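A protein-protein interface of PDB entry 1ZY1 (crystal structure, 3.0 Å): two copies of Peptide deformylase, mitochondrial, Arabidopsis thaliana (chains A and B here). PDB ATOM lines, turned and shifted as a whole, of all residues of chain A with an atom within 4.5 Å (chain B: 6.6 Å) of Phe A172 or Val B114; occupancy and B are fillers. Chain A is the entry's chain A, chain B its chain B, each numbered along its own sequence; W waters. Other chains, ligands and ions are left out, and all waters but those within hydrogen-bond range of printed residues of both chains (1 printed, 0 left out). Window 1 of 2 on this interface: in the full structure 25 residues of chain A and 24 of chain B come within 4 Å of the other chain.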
ATOM      1  N   PHE A 117      11.148   8.835   3.110  1.00  0.00           N
ATOM      2  CA  PHE A 117      10.739   8.740   1.724  1.00  0.00           C
ATOM      3  C   PHE A 117      11.469   7.720   0.865  1.00  0.00           C
ATOM      4  O   PHE A 117      12.654   7.444   1.049  1.00  0.00           O
ATOM      5  CB  PHE A 117      10.866  10.116   1.081  1.00  0.00           C
ATOM      6  CG  PHE A 117       9.921  11.128   1.636  1.00  0.00           C
ATOM      7  CD1 PHE A 117       8.596  11.173   1.198  1.00  0.00           C
ATOM      8  CD2 PHE A 117      10.336  12.007   2.636  1.00  0.00           C
ATOM      9  CE1 PHE A 117       7.705  12.092   1.739  1.00  0.00           C
ATOM     10  CE2 PHE A 117       9.454  12.927   3.185  1.00  0.00           C
ATOM     11  CZ  PHE A 117       8.131  12.968   2.743  1.00  0.00           C
ATOM     12  N   ARG A 118      10.726   7.182  -0.091  1.00  0.00           N
ATOM     13  CA  ARG A 118      11.217   6.202  -1.040  1.00  0.00           C
ATOM     14  C   ARG A 118      10.695   6.668  -2.395  1.00  0.00           C
ATOM     15  O   ARG A 118       9.771   7.477  -2.463  1.00  0.00           O
ATOM     16  CB  ARG A 118      10.656   4.820  -0.701  1.00  0.00           C
ATOM     17  CG  ARG A 118      11.182   4.249   0.610  1.00  0.00           C
ATOM     18  CD  ARG A 118      12.569   3.642   0.412  1.00  0.00           C
ATOM     19  NE  ARG A 118      13.482   3.751   1.518  1.00  0.00           N
ATOM     20  CZ  ARG A 118      13.210   3.910   2.812  1.00  0.00           C
ATOM     21  NH1 ARG A 118      14.098   4.194   3.640  1.00  0.00           N
ATOM     22  NH2 ARG A 118      12.113   3.895   3.362  1.00  0.00           N
ATOM     23  N   ALA A 119      11.293   6.180  -3.470  1.00  0.00           N
ATOM     24  CA  ALA A 119      10.855   6.565  -4.801  1.00  0.00           C
ATOM     25  C   ALA A 119      11.432   5.615  -5.839  1.00  0.00           C
ATOM     26  O   ALA A 119      12.581   5.198  -5.751  1.00  0.00           O
ATOM     27  CB  ALA A 119      11.275   7.997  -5.102  1.00  0.00           C
ATOM     28  N   VAL A 164      16.575  11.535  -5.748  1.00  0.00           N
ATOM     29  CA  VAL A 164      15.461  12.448  -5.999  1.00  0.00           C
ATOM     30  C   VAL A 164      15.530  13.159  -7.344  1.00  0.00           C
ATOM     31  O   VAL A 164      14.492  13.468  -7.932  1.00  0.00           O
ATOM     32  CB  VAL A 164      15.330  13.503  -4.878  1.00  0.00           C
ATOM     33  CG1 VAL A 164      14.943  12.814  -3.573  1.00  0.00           C
ATOM     34  CG2 VAL A 164      16.645  14.270  -4.722  1.00  0.00           C
ATOM     35  N   MET A 167      14.470  10.240  -9.990  1.00  0.00           N
ATOM     36  CA  MET A 167      13.290   9.417  -9.793  1.00  0.00           C
ATOM     37  C   MET A 167      12.234   9.507 -10.871  1.00  0.00           C
ATOM     38  O   MET A 167      12.176  10.473 -11.612  1.00  0.00           O
ATOM     39  CB  MET A 167      12.668   9.724  -8.441  1.00  0.00           C
ATOM     40  CG  MET A 167      12.555  11.183  -8.171  1.00  0.00           C
ATOM     41  SD  MET A 167      12.063  11.426  -6.487  1.00  0.00           S
ATOM     42  CE  MET A 167      10.454  11.598  -6.736  1.00  0.00           C
ATOM     43  N   VAL A 168      11.421   8.459 -10.954  1.00  0.00           N
ATOM     44  CA  VAL A 168      10.325   8.366 -11.903  1.00  0.00           C
ATOM     45  C   VAL A 168       9.218   9.246 -11.347  1.00  0.00           C
ATOM     46  O   VAL A 168       8.771   9.072 -10.207  1.00  0.00           O
ATOM     47  CB  VAL A 168       9.793   6.923 -12.013  1.00  0.00           C
ATOM     48  CG1 VAL A 168       8.630   6.872 -12.981  1.00  0.00           C
ATOM     49  CG2 VAL A 168      10.901   5.993 -12.449  1.00  0.00           C
ATOM     50  N   ARG A 170       6.036  10.975  -9.963  1.00  0.00           N
ATOM     51  CA  ARG A 170       4.889  10.422  -9.250  1.00  0.00           C
ATOM     52  C   ARG A 170       5.114   9.147  -8.455  1.00  0.00           C
ATOM     53  O   ARG A 170       4.153   8.540  -7.980  1.00  0.00           O
ATOM     54  CB  ARG A 170       3.751  10.165 -10.232  1.00  0.00           C
ATOM     55  CG  ARG A 170       3.442  11.335 -11.103  1.00  0.00           C
ATOM     56  CD  ARG A 170       2.296  11.043 -12.035  1.00  0.00           C
ATOM     57  NE  ARG A 170       1.831  12.279 -12.548  1.00  0.00           N
ATOM     58  CZ  ARG A 170       1.436  12.675 -13.747  1.00  0.00           C
ATOM     59  NH1 ARG A 170       1.084  13.936 -13.787  1.00  0.00           N
ATOM     60  NH2 ARG A 170       1.426  11.962 -14.863  1.00  0.00           N
ATOM     61  N   THR A 171       6.357   8.718  -8.305  1.00  0.00           N
ATOM     62  CA  THR A 171       6.582   7.503  -7.535  1.00  0.00           C
ATOM     63  C   THR A 171       7.029   7.895  -6.129  1.00  0.00           C
ATOM     64  O   THR A 171       6.995   7.080  -5.202  1.00  0.00           O
ATOM     65  CB  THR A 171       7.645   6.588  -8.210  1.00  0.00           C
ATOM     66  OG1 THR A 171       8.962   7.104  -7.982  1.00  0.00           O
ATOM     67  CG2 THR A 171       7.403   6.529  -9.702  1.00  0.00           C
ATOM     68  N   PHE A 172       7.437   9.152  -5.973  1.00  0.00           N
ATOM     69  CA  PHE A 172       7.894   9.632  -4.675  1.00  0.00           C
ATOM     70  C   PHE A 172       6.821   9.292  -3.671  1.00  0.00           C
ATOM     71  O   PHE A 172       5.637   9.371  -3.997  1.00  0.00           O
ATOM     72  CB  PHE A 172       8.107  11.146  -4.702  1.00  0.00           C
ATOM     73  CG  PHE A 172       8.983  11.653  -3.591  1.00  0.00           C
ATOM     74  CD1 PHE A 172       8.467  12.476  -2.599  1.00  0.00           C
ATOM     75  CD2 PHE A 172      10.324  11.275  -3.517  1.00  0.00           C
ATOM     76  CE1 PHE A 172       9.275  12.917  -1.535  1.00  0.00           C
ATOM     77  CE2 PHE A 172      11.135  11.708  -2.464  1.00  0.00           C
ATOM     78  CZ  PHE A 172      10.608  12.530  -1.470  1.00  0.00           C
ATOM     79  N   ARG A 173       7.223   8.917  -2.460  1.00  0.00           N
ATOM     80  CA  ARG A 173       6.250   8.559  -1.443  1.00  0.00           C
ATOM     81  C   ARG A 173       6.825   8.329  -0.055  1.00  0.00           C
ATOM     82  O   ARG A 173       8.025   8.111   0.123  1.00  0.00           O
ATOM     83  CB  ARG A 173       5.515   7.292  -1.866  1.00  0.00           C
ATOM     84  CG  ARG A 173       6.417   6.064  -1.972  1.00  0.00           C
ATOM     85  CD  ARG A 173       5.653   4.883  -2.521  1.00  0.00           C
ATOM     86  NE  ARG A 173       5.055   5.214  -3.803  1.00  0.00           N
ATOM     87  CZ  ARG A 173       4.168   4.447  -4.421  1.00  0.00           C
ATOM     88  NH1 ARG A 173       3.790   3.311  -3.862  1.00  0.00           N
ATOM     89  NH2 ARG A 173       3.648   4.811  -5.589  1.00  0.00           N
ATOM     90  N   VAL B   7      -3.203  14.043   2.904  1.00  0.00           N
ATOM     91  CA  VAL B   7      -2.590  12.849   2.359  1.00  0.00           C
ATOM     92  C   VAL B   7      -1.158  13.151   1.982  1.00  0.00           C
ATOM     93  O   VAL B   7      -0.845  14.251   1.539  1.00  0.00           O
ATOM     94  CB  VAL B   7      -3.289  12.354   1.082  1.00  0.00           C
ATOM     95  CG1 VAL B   7      -4.649  12.132   1.279  1.00  0.00           C
ATOM     96  CG2 VAL B   7      -3.219  13.338   0.107  1.00  0.00           C
ATOM     97  N   ALA B   8      -0.306  12.145   2.118  1.00  0.00           N
ATOM     98  CA  ALA B   8       1.093  12.286   1.794  1.00  0.00           C
ATOM     99  C   ALA B   8       1.432  11.496   0.535  1.00  0.00           C
ATOM    100  O   ALA B   8       0.710  10.567   0.170  1.00  0.00           O
ATOM    101  CB  ALA B   8       1.929  11.806   2.954  1.00  0.00           C
ATOM    102  N   SER B   9       2.529  11.859  -0.127  1.00  0.00           N
ATOM    103  CA  SER B   9       2.955  11.167  -1.343  1.00  0.00           C
ATOM    104  C   SER B   9       2.758   9.669  -1.232  1.00  0.00           C
ATOM    105  O   SER B   9       2.982   9.078  -0.179  1.00  0.00           O
ATOM    106  CB  SER B   9       4.428  11.441  -1.637  1.00  0.00           C
ATOM    107  OG  SER B   9       4.605  12.709  -2.220  1.00  0.00           O
ATOM    108  N   GLY B  10       2.354   9.059  -2.336  1.00  0.00           N
ATOM    109  CA  GLY B  10       2.120   7.630  -2.348  1.00  0.00           C
ATOM    110  C   GLY B  10       0.651   7.385  -2.616  1.00  0.00           C
ATOM    111  O   GLY B  10       0.294   6.586  -3.489  1.00  0.00           O
ATOM    112  N   ASP B  11      -0.200   8.084  -1.867  1.00  0.00           N
ATOM    113  CA  ASP B  11      -1.640   7.955  -2.025  1.00  0.00           C
ATOM    114  C   ASP B  11      -2.035   8.406  -3.434  1.00  0.00           C
ATOM    115  O   ASP B  11      -1.998   9.590  -3.756  1.00  0.00           O
ATOM    116  CB  ASP B  11      -2.362   8.808  -0.985  1.00  0.00           C
ATOM    117  CG  ASP B  11      -3.830   8.473  -0.889  1.00  0.00           C
ATOM    118  OD1 ASP B  11      -4.502   8.417  -1.947  1.00  0.00           O
ATOM    119  OD2 ASP B  11      -4.308   8.269   0.251  1.00  0.00           O
ATOM    120  N   HIS B  15      -1.492  11.674  -7.225  1.00  0.00           N
ATOM    121  CA  HIS B  15      -0.775  11.536  -8.473  1.00  0.00           C
ATOM    122  C   HIS B  15      -1.648  11.213  -9.659  1.00  0.00           C
ATOM    123  O   HIS B  15      -1.185  10.610 -10.626  1.00  0.00           O
ATOM    124  CB  HIS B  15       0.324  10.486  -8.323  1.00  0.00           C
ATOM    125  CG  HIS B  15       1.137  10.642  -7.074  1.00  0.00           C
ATOM    126  ND1 HIS B  15       0.792  10.043  -5.882  1.00  0.00           N
ATOM    127  CD2 HIS B  15       2.261  11.352  -6.821  1.00  0.00           C
ATOM    128  CE1 HIS B  15       1.666  10.372  -4.949  1.00  0.00           C
ATOM    129  NE2 HIS B  15       2.569  11.167  -5.493  1.00  0.00           N
ATOM    130  N   GLN B  54      -5.426  16.722  -1.837  1.00  0.00           N
ATOM    131  CA  GLN B  54      -4.664  16.667  -0.596  1.00  0.00           C
ATOM    132  C   GLN B  54      -5.469  16.171   0.612  1.00  0.00           C
ATOM    133  O   GLN B  54      -4.896  15.751   1.618  1.00  0.00           O
ATOM    134  CB  GLN B  54      -4.001  18.024  -0.326  1.00  0.00           C
ATOM    135  CG  GLN B  54      -2.901  18.320  -1.324  1.00  0.00           C
ATOM    136  CD  GLN B  54      -2.066  19.534  -0.962  1.00  0.00           C
ATOM    137  OE1 GLN B  54      -2.548  20.669  -1.005  1.00  0.00           O
ATOM    138  NE2 GLN B  54      -0.800  19.304  -0.600  1.00  0.00           N
ATOM    139  N   GLY B 110       7.523  24.224  -0.854  1.00  0.00           N
ATOM    140  CA  GLY B 110       7.321  23.101   0.041  1.00  0.00           C
ATOM    141  C   GLY B 110       5.873  22.676  -0.062  1.00  0.00           C
ATOM    142  O   GLY B 110       4.990  23.506  -0.269  1.00  0.00           O
ATOM    143  N   CYS B 111       5.616  21.385   0.075  1.00  0.00           N
ATOM    144  CA  CYS B 111       4.259  20.893  -0.018  1.00  0.00           C
ATOM    145  C   CYS B 111       3.890  20.240   1.293  1.00  0.00           C
ATOM    146  O   CYS B 111       4.757  19.747   2.017  1.00  0.00           O
ATOM    147  CB  CYS B 111       4.141  19.891  -1.150  1.00  0.00           C
ATOM    148  SG  CYS B 111       2.480  19.334  -1.444  1.00  0.00           S
ATOM    149  N   LEU B 112       2.599  20.240   1.597  1.00  0.00           N
ATOM    150  CA  LEU B 112       2.109  19.667   2.841  1.00  0.00           C
ATOM    151  C   LEU B 112       2.026  18.150   2.742  1.00  0.00           C
ATOM    152  O   LEU B 112       1.859  17.453   3.741  1.00  0.00           O
ATOM    153  CB  LEU B 112       0.745  20.281   3.162  1.00  0.00           C
ATOM    154  CG  LEU B 112       0.818  21.813   3.071  1.00  0.00           C
ATOM    155  CD1 LEU B 112      -0.574  22.413   3.081  1.00  0.00           C
ATOM    156  CD2 LEU B 112       1.654  22.352   4.215  1.00  0.00           C
ATOM    157  N   SER B 113       2.163  17.643   1.523  1.00  0.00           N
ATOM    158  CA  SER B 113       2.123  16.206   1.279  1.00  0.00           C
ATOM    159  C   SER B 113       3.553  15.660   1.203  1.00  0.00           C
ATOM    160  O   SER B 113       3.771  14.470   0.975  1.00  0.00           O
ATOM    161  CB  SER B 113       1.368  15.922  -0.025  1.00  0.00           C
ATOM    162  OG  SER B 113       0.057  16.474   0.015  1.00  0.00           O
ATOM    163  N   VAL B 114       4.518  16.557   1.399  1.00  0.00           N
ATOM    164  CA  VAL B 114       5.948  16.231   1.389  1.00  0.00           C
ATOM    165  C   VAL B 114       6.579  17.148   2.418  1.00  0.00           C
ATOM    166  O   VAL B 114       7.304  18.091   2.065  1.00  0.00           O
ATOM    167  CB  VAL B 114       6.622  16.550   0.032  1.00  0.00           C
ATOM    168  CG1 VAL B 114       8.080  16.133   0.073  1.00  0.00           C
ATOM    169  CG2 VAL B 114       5.886  15.862  -1.089  1.00  0.00           C
ATOM    170  N   ASP B 115       6.303  16.883   3.687  1.00  0.00           N
ATOM    171  CA  ASP B 115       6.824  17.752   4.724  1.00  0.00           C
ATOM    172  C   ASP B 115       8.182  17.340   5.249  1.00  0.00           C
ATOM    173  O   ASP B 115       8.539  16.162   5.239  1.00  0.00           O
ATOM    174  CB  ASP B 115       5.844  17.835   5.884  1.00  0.00           C
ATOM    175  CG  ASP B 115       5.939  16.653   6.784  1.00  0.00           C
ATOM    176  OD1 ASP B 115       5.886  15.522   6.254  1.00  0.00           O
ATOM    177  OD2 ASP B 115       6.075  16.853   8.009  1.00  0.00           O
ATOM    178  N   GLY B 116       8.921  18.340   5.723  1.00  0.00           N
ATOM    179  CA  GLY B 116      10.253  18.136   6.254  1.00  0.00           C
ATOM    180  C   GLY B 116      11.220  18.519   5.164  1.00  0.00           C
ATOM    181  O   GLY B 116      12.422  18.626   5.400  1.00  0.00           O
ATOM    182  N   PHE B 117      10.678  18.751   3.971  1.00  0.00           N
ATOM    183  CA  PHE B 117      11.493  19.089   2.820  1.00  0.00           C
ATOM    184  C   PHE B 117      11.050  20.272   1.989  1.00  0.00           C
ATOM    185  O   PHE B 117       9.859  20.555   1.842  1.00  0.00           O
ATOM    186  CB  PHE B 117      11.599  17.868   1.925  1.00  0.00           C
ATOM    187  CG  PHE B 117      12.359  16.738   2.546  1.00  0.00           C
ATOM    188  CD1 PHE B 117      13.752  16.733   2.540  1.00  0.00           C
ATOM    189  CD2 PHE B 117      11.687  15.694   3.170  1.00  0.00           C
ATOM    190  CE1 PHE B 117      14.453  15.688   3.122  1.00  0.00           C
ATOM    191  CE2 PHE B 117      12.384  14.648   3.755  1.00  0.00           C
ATOM    192  CZ  PHE B 117      13.765  14.650   3.740  1.00  0.00           C
ATOM    193  N   ARG B 118      12.037  20.960   1.433  1.00  0.00           N
ATOM    194  CA  ARG B 118      11.810  22.119   0.570  1.00  0.00           C
ATOM    195  C   ARG B 118      12.734  21.912  -0.615  1.00  0.00           C
ATOM    196  O   ARG B 118      13.667  21.095  -0.537  1.00  0.00           O
ATOM    197  CB  ARG B 118      12.207  23.404   1.314  1.00  0.00           C
ATOM    198  CG  ARG B 118      11.273  23.769   2.457  1.00  0.00           C
ATOM    199  CD  ARG B 118       9.891  24.145   1.909  1.00  0.00           C
ATOM    200  NE  ARG B 118       9.037  24.507   3.033  1.00  0.00           N
ATOM    201  CZ  ARG B 118       8.558  23.713   3.981  1.00  0.00           C
ATOM    202  NH1 ARG B 118       8.655  22.447   4.055  1.00  0.00           N
ATOM    203  NH2 ARG B 118       8.394  24.194   5.142  1.00  0.00           N
ATOM    204  N   LEU B 162       3.534  16.999  -8.205  1.00  0.00           N
ATOM    205  CA  LEU B 162       4.139  17.588  -7.019  1.00  0.00           C
ATOM    206  C   LEU B 162       5.446  18.232  -7.460  1.00  0.00           C
ATOM    207  O   LEU B 162       6.052  17.799  -8.443  1.00  0.00           O
ATOM    208  CB  LEU B 162       4.412  16.532  -5.956  1.00  0.00           C
ATOM    209  CG  LEU B 162       3.208  15.709  -5.496  1.00  0.00           C
ATOM    210  CD1 LEU B 162       3.627  14.887  -4.305  1.00  0.00           C
ATOM    211  CD2 LEU B 162       2.034  16.610  -5.126  1.00  0.00           C
ATOM    212  N   TYR B 163       5.879  19.265  -6.740  1.00  0.00           N
ATOM    213  CA  TYR B 163       7.095  19.979  -7.105  1.00  0.00           C
ATOM    214  C   TYR B 163       8.299  19.080  -7.253  1.00  0.00           C
ATOM    215  O   TYR B 163       9.184  19.368  -8.056  1.00  0.00           O
ATOM    216  CB  TYR B 163       7.415  21.063  -6.081  1.00  0.00           C
ATOM    217  CG  TYR B 163       7.768  20.558  -4.692  1.00  0.00           C
ATOM    218  CD1 TYR B 163       9.100  20.512  -4.251  1.00  0.00           C
ATOM    219  CD2 TYR B 163       6.769  20.203  -3.792  1.00  0.00           C
ATOM    220  CE1 TYR B 163       9.421  20.131  -2.929  1.00  0.00           C
ATOM    221  CE2 TYR B 163       7.073  19.825  -2.476  1.00  0.00           C
ATOM    222  CZ  TYR B 163       8.395  19.795  -2.046  1.00  0.00           C
ATOM    223  OH  TYR B 163       8.680  19.476  -0.738  1.00  0.00           O
ATOM    224  N   VAL B 164       8.347  17.992  -6.493  1.00  0.00           N
ATOM    225  CA  VAL B 164       9.497  17.104  -6.560  1.00  0.00           C
ATOM    226  C   VAL B 164       9.887  16.694  -7.986  1.00  0.00           C
ATOM    227  O   VAL B 164      11.073  16.492  -8.294  1.00  0.00           O
ATOM    228  CB  VAL B 164       9.279  15.844  -5.678  1.00  0.00           C
ATOM    229  CG1 VAL B 164       9.222  16.252  -4.215  1.00  0.00           C
ATOM    230  CG2 VAL B 164       8.004  15.118  -6.082  1.00  0.00           C
ATOM    231  N   ASP B 165       8.905  16.593  -8.870  1.00  0.00           N
ATOM    232  CA  ASP B 165       9.216  16.196 -10.230  1.00  0.00           C
ATOM    233  C   ASP B 165       9.442  17.415 -11.113  1.00  0.00           C
ATOM    234  O   ASP B 165       9.502  17.298 -12.331  1.00  0.00           O
ATOM    235  CB  ASP B 165       8.098  15.308 -10.783  1.00  0.00           C
ATOM    236  CG  ASP B 165       7.827  14.086  -9.900  1.00  0.00           C
ATOM    237  OD1 ASP B 165       8.753  13.281  -9.676  1.00  0.00           O
ATOM    238  OD2 ASP B 165       6.679  13.934  -9.424  1.00  0.00           O
ATOM    239  N   PHE B 172      17.012  20.038  -3.396  1.00  0.00           N
ATOM    240  CA  PHE B 172      16.198  19.326  -2.425  1.00  0.00           C
ATOM    241  C   PHE B 172      16.901  19.409  -1.091  1.00  0.00           C
ATOM    242  O   PHE B 172      18.126  19.309  -1.032  1.00  0.00           O
ATOM    243  CB  PHE B 172      16.046  17.860  -2.803  1.00  0.00           C
ATOM    244  CG  PHE B 172      14.887  17.178  -2.132  1.00  0.00           C
ATOM    245  CD1 PHE B 172      15.096  16.173  -1.196  1.00  0.00           C
ATOM    246  CD2 PHE B 172      13.581  17.572  -2.413  1.00  0.00           C
ATOM    247  CE1 PHE B 172      14.012  15.559  -0.559  1.00  0.00           C
ATOM    248  CE2 PHE B 172      12.501  16.967  -1.783  1.00  0.00           C
ATOM    249  CZ  PHE B 172      12.716  15.963  -0.847  1.00  0.00           C
HETATM  250  O   HOH W   1      11.114  13.305 -11.247  1.00  0.00           O
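Among the printed residues, merely in contact across the chains: Phe A172 with Ser B9 (3.4 Å), Arg A173 with Ser B9 (3.4 Å), Phe A117 with Phe B117 (3.4 Å), Arg A173 with Gly B10 (3.4 Å), Arg A170 with His B15 (3.6 Å), Phe A172 with Gly B10 (3.7 Å), Phe A172 with Val B114 (3.8 Å), Met A167 with Asp B165 (3.8 Å), Phe A172 with His B15 (3.9 Å) and Phe A117 with Asp B115 (3.9 Å).
O of Arg A173 lies within hydrogen-bond range of N of Arg A118 (2.9 Å).
The guanidinium group (NE) of Arg A173 lies within hydrogen-bond range of the backbone carbonyl oxygen (O) of Thr A171 (3.0 Å).
The backbone NH of Ser B9 sits at hydrogen-bond distance from the backbone carbonyl oxygen of Ser B113 (3.1 Å).
OH of Tyr B163 is in hydrogen-bond range of O of Val B114 (3.4 Å).
The backbone carbonyl oxygen (O) of Phe B117 is in hydrogen-bond range of the side-chain hydroxyl (OH) of Tyr B163 (3.0 Å).
The backbone NH of Arg A170 is in hydrogen-bond range of the side-chain carboxylate of Asp B165 (3.1 Å).
Water W1 lies within hydrogen-bond range of the side-chain carboxylate of Asp B165 (2.8 Å) and the backbone carbonyl oxygen of Met A167 (3.0 Å).
Of chain B, only Ser B9 (3.4 Å), Gly B10 (3.7 Å), His B15 (3.9 Å) and Val B114 (3.8 Å) come within 4 Å of Phe A172.
Of chain A, only Phe A172 (3.8 Å) comes within 4 Å of Val B114.
Of the printed residues of chain A, Asp B165 touches Met A167 and Arg A170.
Printed residues of chain A within 4 Å of Ser B9: Phe A172 and Arg A173.
Of the printed residues of chain B, Phe A117 touches Asp B115 and Phe B117.
Ser B113 touches none of the printed residues of chain A.
Arg A118 touches none of the printed residues of chain B.
The nearest residue of chain B that does not touch Phe A172 is Phe B172 (4.1 Å).
The nearest residue of chain A that does not touch Val B114 is Phe A117 (4.1 Å).
The nearest printed residue of chain A that does not touch Asp B165 is Val A168 (4.2 Å).
Phe A117 touches its own counterpart, Phe B117.
Of the 11 pairs that touch across the chains among the printed residues, 1 has its exchanged pair printed and touching as well.
Of the 10 printed residues of chain A, 5 touch a printed residue of chain B.
Hydrophobic or aromatic side chains of chain B that line the printed part of chain A: His B15, Val B114 and Phe B117.
Among the printed residues, 11 pairs touch across the chains.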
